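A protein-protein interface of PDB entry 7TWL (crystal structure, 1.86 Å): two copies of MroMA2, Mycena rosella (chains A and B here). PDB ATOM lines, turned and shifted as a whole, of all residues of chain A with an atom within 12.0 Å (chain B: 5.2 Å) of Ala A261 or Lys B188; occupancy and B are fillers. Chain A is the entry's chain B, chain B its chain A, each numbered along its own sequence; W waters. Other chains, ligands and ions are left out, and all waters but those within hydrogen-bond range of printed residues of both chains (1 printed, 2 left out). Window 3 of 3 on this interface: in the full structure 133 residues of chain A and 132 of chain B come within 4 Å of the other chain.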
ATOM      1  N   ILE A 254      30.621 -20.864  35.453  1.00  0.00           N
ATOM      2  CA  ILE A 254      29.888 -21.607  34.437  1.00  0.00           C
ATOM      3  C   ILE A 254      29.881 -23.085  34.832  1.00  0.00           C
ATOM      4  O   ILE A 254      30.938 -23.692  34.963  1.00  0.00           O
ATOM      5  CB  ILE A 254      30.556 -21.402  33.059  1.00  0.00           C
ATOM      6  CG1 ILE A 254      30.755 -19.922  32.708  1.00  0.00           C
ATOM      7  CG2 ILE A 254      29.823 -22.164  31.961  1.00  0.00           C
ATOM      8  CD1 ILE A 254      29.498 -19.196  32.267  1.00  0.00           C
ATOM      9  N   ASP A 255      28.691 -23.660  35.029  1.00  0.00           N
ATOM     10  CA  ASP A 255      28.597 -25.053  35.436  1.00  0.00           C
ATOM     11  C   ASP A 255      28.675 -25.947  34.193  1.00  0.00           C
ATOM     12  O   ASP A 255      27.766 -25.927  33.361  1.00  0.00           O
ATOM     13  CB  ASP A 255      27.374 -25.273  36.334  1.00  0.00           C
ATOM     14  CG  ASP A 255      27.031 -26.727  36.643  1.00  0.00           C
ATOM     15  OD1 ASP A 255      27.699 -27.635  36.102  1.00  0.00           O
ATOM     16  OD2 ASP A 255      26.087 -26.942  37.432  1.00  0.00           O
ATOM     17  N   PRO A 256      29.733 -26.788  34.044  1.00  0.00           N
ATOM     18  CA  PRO A 256      29.907 -27.612  32.844  1.00  0.00           C
ATOM     19  C   PRO A 256      28.729 -28.541  32.555  1.00  0.00           C
ATOM     20  O   PRO A 256      28.438 -28.810  31.393  1.00  0.00           O
ATOM     21  CB  PRO A 256      31.183 -28.431  33.122  1.00  0.00           C
ATOM     22  CG  PRO A 256      31.913 -27.621  34.175  1.00  0.00           C
ATOM     23  CD  PRO A 256      30.815 -27.007  35.023  1.00  0.00           C
ATOM     24  N   LYS A 257      28.040 -29.002  33.607  1.00  0.00           N
ATOM     25  CA  LYS A 257      26.872 -29.858  33.448  1.00  0.00           C
ATOM     26  C   LYS A 257      25.686 -29.077  32.887  1.00  0.00           C
ATOM     27  O   LYS A 257      24.869 -29.634  32.157  1.00  0.00           O
ATOM     28  CB  LYS A 257      26.469 -30.496  34.778  1.00  0.00           C
ATOM     29  CG  LYS A 257      27.417 -31.583  35.277  1.00  0.00           C
ATOM     30  CD  LYS A 257      26.965 -32.228  36.571  1.00  0.00           C
ATOM     31  CE  LYS A 257      25.646 -32.964  36.446  1.00  0.00           C
ATOM     32  NZ  LYS A 257      25.285 -33.654  37.707  1.00  0.00           N
ATOM     33  N   ALA A 258      25.562 -27.805  33.285  1.00  0.00           N
ATOM     34  CA  ALA A 258      24.523 -26.941  32.746  1.00  0.00           C
ATOM     35  C   ALA A 258      24.811 -26.637  31.276  1.00  0.00           C
ATOM     36  O   ALA A 258      23.885 -26.619  30.464  1.00  0.00           O
ATOM     37  CB  ALA A 258      24.387 -25.680  33.576  1.00  0.00           C
ATOM     38  N   VAL A 259      26.096 -26.431  30.944  1.00  0.00           N
ATOM     39  CA  VAL A 259      26.546 -26.207  29.574  1.00  0.00           C
ATOM     40  C   VAL A 259      26.066 -27.361  28.694  1.00  0.00           C
ATOM     41  O   VAL A 259      25.491 -27.124  27.628  1.00  0.00           O
ATOM     42  CB  VAL A 259      28.074 -25.991  29.499  1.00  0.00           C
ATOM     43  CG1 VAL A 259      28.638 -26.072  28.085  1.00  0.00           C
ATOM     44  CG2 VAL A 259      28.495 -24.684  30.155  1.00  0.00           C
ATOM     45  N   GLN A 260      26.257 -28.602  29.181  1.00  0.00           N
ATOM     46  CA  GLN A 260      25.809 -29.801  28.490  1.00  0.00           C
ATOM     47  C   GLN A 260      24.298 -29.792  28.289  1.00  0.00           C
ATOM     48  O   GLN A 260      23.820 -30.000  27.177  1.00  0.00           O
ATOM     49  CB  GLN A 260      26.103 -31.066  29.299  1.00  0.00           C
ATOM     50  CG  GLN A 260      27.018 -32.045  28.596  1.00  0.00           C
ATOM     51  CD  GLN A 260      26.661 -32.277  27.149  1.00  0.00           C
ATOM     52  OE1 GLN A 260      27.500 -32.122  26.283  1.00  0.00           O
ATOM     53  NE2 GLN A 260      25.426 -32.662  26.880  1.00  0.00           N
ATOM     54  N   ALA A 261      23.553 -29.614  29.389  1.00  0.00           N
ATOM     55  CA  ALA A 261      22.099 -29.685  29.345  1.00  0.00           C
ATOM     56  C   ALA A 261      21.551 -28.639  28.374  1.00  0.00           C
ATOM     57  O   ALA A 261      20.511 -28.854  27.753  1.00  0.00           O
ATOM     58  CB  ALA A 261      21.517 -29.498  30.725  1.00  0.00           C
ATOM     59  N   LEU A 262      22.266 -27.515  28.254  1.00  0.00           N
ATOM     60  CA  LEU A 262      21.802 -26.393  27.455  1.00  0.00           C
ATOM     61  C   LEU A 262      22.159 -26.582  25.982  1.00  0.00           C
ATOM     62  O   LEU A 262      21.592 -25.912  25.117  1.00  0.00           O
ATOM     63  CB  LEU A 262      22.367 -25.089  28.027  1.00  0.00           C
ATOM     64  CG  LEU A 262      21.565 -24.509  29.195  1.00  0.00           C
ATOM     65  CD1 LEU A 262      22.455 -23.676  30.097  1.00  0.00           C
ATOM     66  CD2 LEU A 262      20.420 -23.646  28.686  1.00  0.00           C
ATOM     67  N   GLY A 263      23.062 -27.530  25.700  1.00  0.00           N
ATOM     68  CA  GLY A 263      23.484 -27.791  24.333  1.00  0.00           C
ATOM     69  C   GLY A 263      24.503 -26.769  23.839  1.00  0.00           C
ATOM     70  O   GLY A 263      24.626 -26.535  22.635  1.00  0.00           O
ATOM     71  N   LEU A 264      25.272 -26.197  24.771  1.00  0.00           N
ATOM     72  CA  LEU A 264      26.250 -25.182  24.425  1.00  0.00           C
ATOM     73  C   LEU A 264      27.621 -25.838  24.264  1.00  0.00           C
ATOM     74  O   LEU A 264      27.837 -26.927  24.799  1.00  0.00           O
ATOM     75  CB  LEU A 264      26.252 -24.107  25.519  1.00  0.00           C
ATOM     76  CG  LEU A 264      25.051 -23.153  25.507  1.00  0.00           C
ATOM     77  CD1 LEU A 264      24.963 -22.384  26.814  1.00  0.00           C
ATOM     78  CD2 LEU A 264      25.144 -22.180  24.342  1.00  0.00           C
ATOM     79  N   PRO A 265      28.567 -25.207  23.520  1.00  0.00           N
ATOM     80  CA  PRO A 265      29.906 -25.769  23.305  1.00  0.00           C
ATOM     81  C   PRO A 265      30.649 -26.114  24.595  1.00  0.00           C
ATOM     82  O   PRO A 265      30.692 -25.320  25.536  1.00  0.00           O
ATOM     83  CB  PRO A 265      30.661 -24.650  22.575  1.00  0.00           C
ATOM     84  CG  PRO A 265      29.578 -23.843  21.888  1.00  0.00           C
ATOM     85  CD  PRO A 265      28.384 -23.926  22.817  1.00  0.00           C
ATOM     86  N   ALA A 266      31.258 -27.305  24.608  1.00  0.00           N
ATOM     87  CA  ALA A 266      31.865 -27.867  25.803  1.00  0.00           C
ATOM     88  C   ALA A 266      33.063 -27.029  26.243  1.00  0.00           C
ATOM     89  O   ALA A 266      33.732 -26.390  25.433  1.00  0.00           O
ATOM     90  CB  ALA A 266      32.255 -29.304  25.552  1.00  0.00           C
ATOM     91  N   THR A 267      33.298 -27.036  27.557  1.00  0.00           N
ATOM     92  CA  THR A 267      34.449 -26.402  28.183  1.00  0.00           C
ATOM     93  C   THR A 267      34.512 -24.917  27.838  1.00  0.00           C
ATOM     94  O   THR A 267      35.530 -24.273  28.093  1.00  0.00           O
ATOM     95  CB  THR A 267      35.768 -27.133  27.883  1.00  0.00           C
ATOM     96  OG1 THR A 267      35.534 -28.534  27.714  1.00  0.00           O
ATOM     97  CG2 THR A 267      36.806 -26.908  28.963  1.00  0.00           C
ATOM     98  N   VAL A 268      33.428 -24.377  27.260  1.00  0.00           N
ATOM     99  CA  VAL A 268      33.303 -22.929  27.208  1.00  0.00           C
ATOM    100  C   VAL A 268      33.284 -22.429  28.652  1.00  0.00           C
ATOM    101  O   VAL A 268      32.441 -22.832  29.454  1.00  0.00           O
ATOM    102  CB  VAL A 268      32.130 -22.416  26.339  1.00  0.00           C
ATOM    103  CG1 VAL A 268      30.760 -22.557  26.994  1.00  0.00           C
ATOM    104  CG2 VAL A 268      32.363 -20.985  25.876  1.00  0.00           C
ATOM    105  N   ILE A 398      25.320 -15.472  26.111  1.00  0.00           N
ATOM    106  CA  ILE A 398      25.961 -15.347  27.417  1.00  0.00           C
ATOM    107  C   ILE A 398      27.286 -16.112  27.469  1.00  0.00           C
ATOM    108  O   ILE A 398      28.078 -15.894  28.384  1.00  0.00           O
ATOM    109  CB  ILE A 398      25.020 -15.653  28.600  1.00  0.00           C
ATOM    110  CG1 ILE A 398      24.402 -17.048  28.485  1.00  0.00           C
ATOM    111  CG2 ILE A 398      23.961 -14.569  28.730  1.00  0.00           C
ATOM    112  CD1 ILE A 398      25.389 -18.171  28.682  1.00  0.00           C
ATOM    113  N   VAL A 399      27.524 -16.991  26.484  1.00  0.00           N
ATOM    114  CA  VAL A 399      28.846 -17.573  26.283  1.00  0.00           C
ATOM    115  C   VAL A 399      29.388 -17.125  24.915  1.00  0.00           C
ATOM    116  O   VAL A 399      30.623 -16.918  24.825  1.00  0.00           O
ATOM    117  CB  VAL A 399      28.845 -19.108  26.419  1.00  0.00           C
ATOM    118  CG1 VAL A 399      28.455 -19.563  27.819  1.00  0.00           C
ATOM    119  CG2 VAL A 399      27.993 -19.789  25.354  1.00  0.00           C
ATOM    120  N   VAL B 177      16.645 -20.098  24.900  1.00  0.00           N
ATOM    121  CA  VAL B 177      17.341 -20.814  25.946  1.00  0.00           C
ATOM    122  C   VAL B 177      18.330 -21.773  25.278  1.00  0.00           C
ATOM    123  O   VAL B 177      17.914 -22.638  24.505  1.00  0.00           O
ATOM    124  CB  VAL B 177      16.359 -21.565  26.859  1.00  0.00           C
ATOM    125  CG1 VAL B 177      17.114 -22.369  27.901  1.00  0.00           C
ATOM    126  CG2 VAL B 177      15.376 -20.612  27.547  1.00  0.00           C
ATOM    127  N   GLY B 178      19.627 -21.573  25.559  1.00  0.00           N
ATOM    128  CA  GLY B 178      20.668 -22.503  25.140  1.00  0.00           C
ATOM    129  C   GLY B 178      21.076 -22.337  23.675  1.00  0.00           C
ATOM    130  O   GLY B 178      21.906 -23.099  23.170  1.00  0.00           O
ATOM    131  N   ASP B 185      13.960 -22.737  18.343  1.00  0.00           N
ATOM    132  CA  ASP B 185      12.911 -23.738  18.227  1.00  0.00           C
ATOM    133  C   ASP B 185      12.290 -24.061  19.589  1.00  0.00           C
ATOM    134  O   ASP B 185      11.411 -24.921  19.681  1.00  0.00           O
ATOM    135  CB  ASP B 185      13.441 -24.993  17.524  1.00  0.00           C
ATOM    136  CG  ASP B 185      14.439 -25.801  18.347  1.00  0.00           C
ATOM    137  OD1 ASP B 185      14.896 -25.307  19.407  1.00  0.00           O
ATOM    138  OD2 ASP B 185      14.768 -26.920  17.914  1.00  0.00           O
ATOM    139  N   ASN B 186      12.753 -23.376  20.646  1.00  0.00           N
ATOM    140  CA  ASN B 186      12.248 -23.555  22.003  1.00  0.00           C
ATOM    141  C   ASN B 186      12.577 -24.941  22.552  1.00  0.00           C
ATOM    142  O   ASN B 186      11.944 -25.397  23.503  1.00  0.00           O
ATOM    143  CB  ASN B 186      10.760 -23.221  22.134  1.00  0.00           C
ATOM    144  CG  ASN B 186      10.527 -21.732  22.291  1.00  0.00           C
ATOM    145  OD1 ASN B 186       9.464 -21.220  21.932  1.00  0.00           O
ATOM    146  ND2 ASN B 186      11.519 -21.033  22.810  1.00  0.00           N
ATOM    147  N   GLY B 187      13.604 -25.579  21.977  1.00  0.00           N
ATOM    148  CA  GLY B 187      13.934 -26.952  22.336  1.00  0.00           C
ATOM    149  C   GLY B 187      14.394 -27.070  23.790  1.00  0.00           C
ATOM    150  O   GLY B 187      14.243 -28.131  24.402  1.00  0.00           O
ATOM    151  N   LYS B 188      14.942 -25.969  24.340  1.00  0.00           N
ATOM    152  CA  LYS B 188      15.468 -25.978  25.697  1.00  0.00           C
ATOM    153  C   LYS B 188      14.608 -25.148  26.663  1.00  0.00           C
ATOM    154  O   LYS B 188      14.996 -24.950  27.826  1.00  0.00           O
ATOM    155  CB  LYS B 188      16.942 -25.553  25.720  1.00  0.00           C
ATOM    156  CG  LYS B 188      17.886 -26.354  24.822  1.00  0.00           C
ATOM    157  CD  LYS B 188      17.762 -27.842  25.027  1.00  0.00           C
ATOM    158  CE  LYS B 188      18.900 -28.640  24.423  1.00  0.00           C
ATOM    159  NZ  LYS B 188      18.862 -30.024  24.949  1.00  0.00           N
ATOM    160  N   PHE B 189      13.419 -24.719  26.211  1.00  0.00           N
ATOM    161  CA  PHE B 189      12.542 -23.901  27.043  1.00  0.00           C
ATOM    162  C   PHE B 189      12.158 -24.642  28.338  1.00  0.00           C
ATOM    163  O   PHE B 189      12.077 -24.039  29.416  1.00  0.00           O
ATOM    164  CB  PHE B 189      11.327 -23.415  26.245  1.00  0.00           C
ATOM    165  CG  PHE B 189      10.357 -22.587  27.055  1.00  0.00           C
ATOM    166  CD1 PHE B 189      10.623 -21.251  27.329  1.00  0.00           C
ATOM    167  CD2 PHE B 189       9.190 -23.145  27.555  1.00  0.00           C
ATOM    168  CE1 PHE B 189       9.735 -20.491  28.083  1.00  0.00           C
ATOM    169  CE2 PHE B 189       8.295 -22.384  28.296  1.00  0.00           C
ATOM    170  CZ  PHE B 189       8.584 -21.060  28.572  1.00  0.00           C
ATOM    171  N   HIS B 190      11.963 -25.962  28.241  1.00  0.00           N
ATOM    172  CA  HIS B 190      11.542 -26.753  29.388  1.00  0.00           C
ATOM    173  C   HIS B 190      12.507 -26.627  30.568  1.00  0.00           C
ATOM    174  O   HIS B 190      12.082 -26.796  31.709  1.00  0.00           O
ATOM    175  CB  HIS B 190      11.277 -28.220  29.003  1.00  0.00           C
ATOM    176  CG  HIS B 190      12.524 -28.963  28.660  1.00  0.00           C
ATOM    177  ND1 HIS B 190      13.126 -28.858  27.421  1.00  0.00           N
ATOM    178  CD2 HIS B 190      13.292 -29.805  29.388  1.00  0.00           C
ATOM    179  CE1 HIS B 190      14.214 -29.607  27.395  1.00  0.00           C
ATOM    180  NE2 HIS B 190      14.331 -30.199  28.590  1.00  0.00           N
ATOM    181  N   LEU B 191      13.791 -26.345  30.302  1.00  0.00           N
ATOM    182  CA  LEU B 191      14.766 -26.172  31.370  1.00  0.00           C
ATOM    183  C   LEU B 191      14.404 -24.950  32.223  1.00  0.00           C
ATOM    184  O   LEU B 191      14.553 -24.981  33.446  1.00  0.00           O
ATOM    185  CB  LEU B 191      16.183 -26.053  30.790  1.00  0.00           C
ATOM    186  CG  LEU B 191      16.747 -27.313  30.121  1.00  0.00           C
ATOM    187  CD1 LEU B 191      18.163 -27.058  29.615  1.00  0.00           C
ATOM    188  CD2 LEU B 191      16.745 -28.494  31.093  1.00  0.00           C
ATOM    189  N   LEU B 192      13.931 -23.878  31.571  1.00  0.00           N
ATOM    190  CA  LEU B 192      13.496 -22.692  32.303  1.00  0.00           C
ATOM    191  C   LEU B 192      12.208 -23.000  33.079  1.00  0.00           C
ATOM    192  O   LEU B 192      12.037 -22.542  34.205  1.00  0.00           O
ATOM    193  CB  LEU B 192      13.314 -21.521  31.322  1.00  0.00           C
ATOM    194  CG  LEU B 192      12.838 -20.208  31.953  1.00  0.00           C
ATOM    195  CD1 LEU B 192      13.861 -19.657  32.942  1.00  0.00           C
ATOM    196  CD2 LEU B 192      12.499 -19.166  30.891  1.00  0.00           C
HETATM  197  O   HOH W   1      18.828 -30.866  28.294  1.00  0.00           O
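Ala A261 touches just these residues of chain B: Lys B188 and Leu B191. Of the printed residues of chain B, Leu A262 touches Val B177, Gly B178 and Lys B188. Of the printed residues of chain B, Leu A264 touches Gly B178. Val B177 touches just one residue of chain A: Leu A262 (3.6 Å). Gly B178 touches just these residues of chain A: Leu A262 (3.4 Å) and Leu A264 (3.6 Å). No residue of chain A comes within 4 Å of Asp B185. No residue of chain A comes within 4 Å of Gly B187. Of chain A, only Ala A261 (3.5 Å) and Leu A262 (3.7 Å) come within 4 Å of Lys B188. No residue of chain A comes within 4 Å of Phe B189. No residue of chain A comes within 4 Å of His B190. No residue of chain A comes within 4 Å of Leu B192. The nearest printed residue of chain B that does not touch Ala A261 is His B190 (6.4 Å). The nearest residue of chain A that does not touch Lys B188 is Gly A263 (4.5 Å). The nearest printed residue of chain B that does not touch Leu A264 is Lys B188 (6.8 Å).
Leu B191 touches Ala A261. Leu A262 touches Val B177 (CD2 to CG1, 3.6 Å). Leu A262 touches Lys B188. Gly B178 touches Leu A264 (O to CD2, 3.6 Å).
The backbone carbonyl oxygen (O) of Val A259 sits at hydrogen-bond distance from the backbone NH (N) of Leu A264 (3.0 Å).
No position is printed for both chains. Of the 6 pairs that touch across the chains among the printed residues, none has its exchanged pair printed and touching as well.
O of Ala A261 is in hydrogen-bond range of NZ of Lys B188 (3.5 Å). O of Leu A262 lies close to O of Gly B178 (3.4 Å).
Printed residues of chain A that touch a printed residue of chain B: Ala A261, Leu A262 and Leu A264. Hydrophobic or aromatic side chains of chain A that line the printed part of chain B: Leu A262 and Leu A264. Hydrophobic or aromatic side chains of chain B within 4 Å of the printed part of chain A: Val B177 and Leu B191. Along chain B the printed residues that touch a printed residue of chain A span positions 177 to 191. Among the printed residues, 6 pairs touch across the chains.
Water W1 lies within hydrogen-bond range of O of Ala A261 (2.7 Å) and NZ of Lys B188 (3.4 Å).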
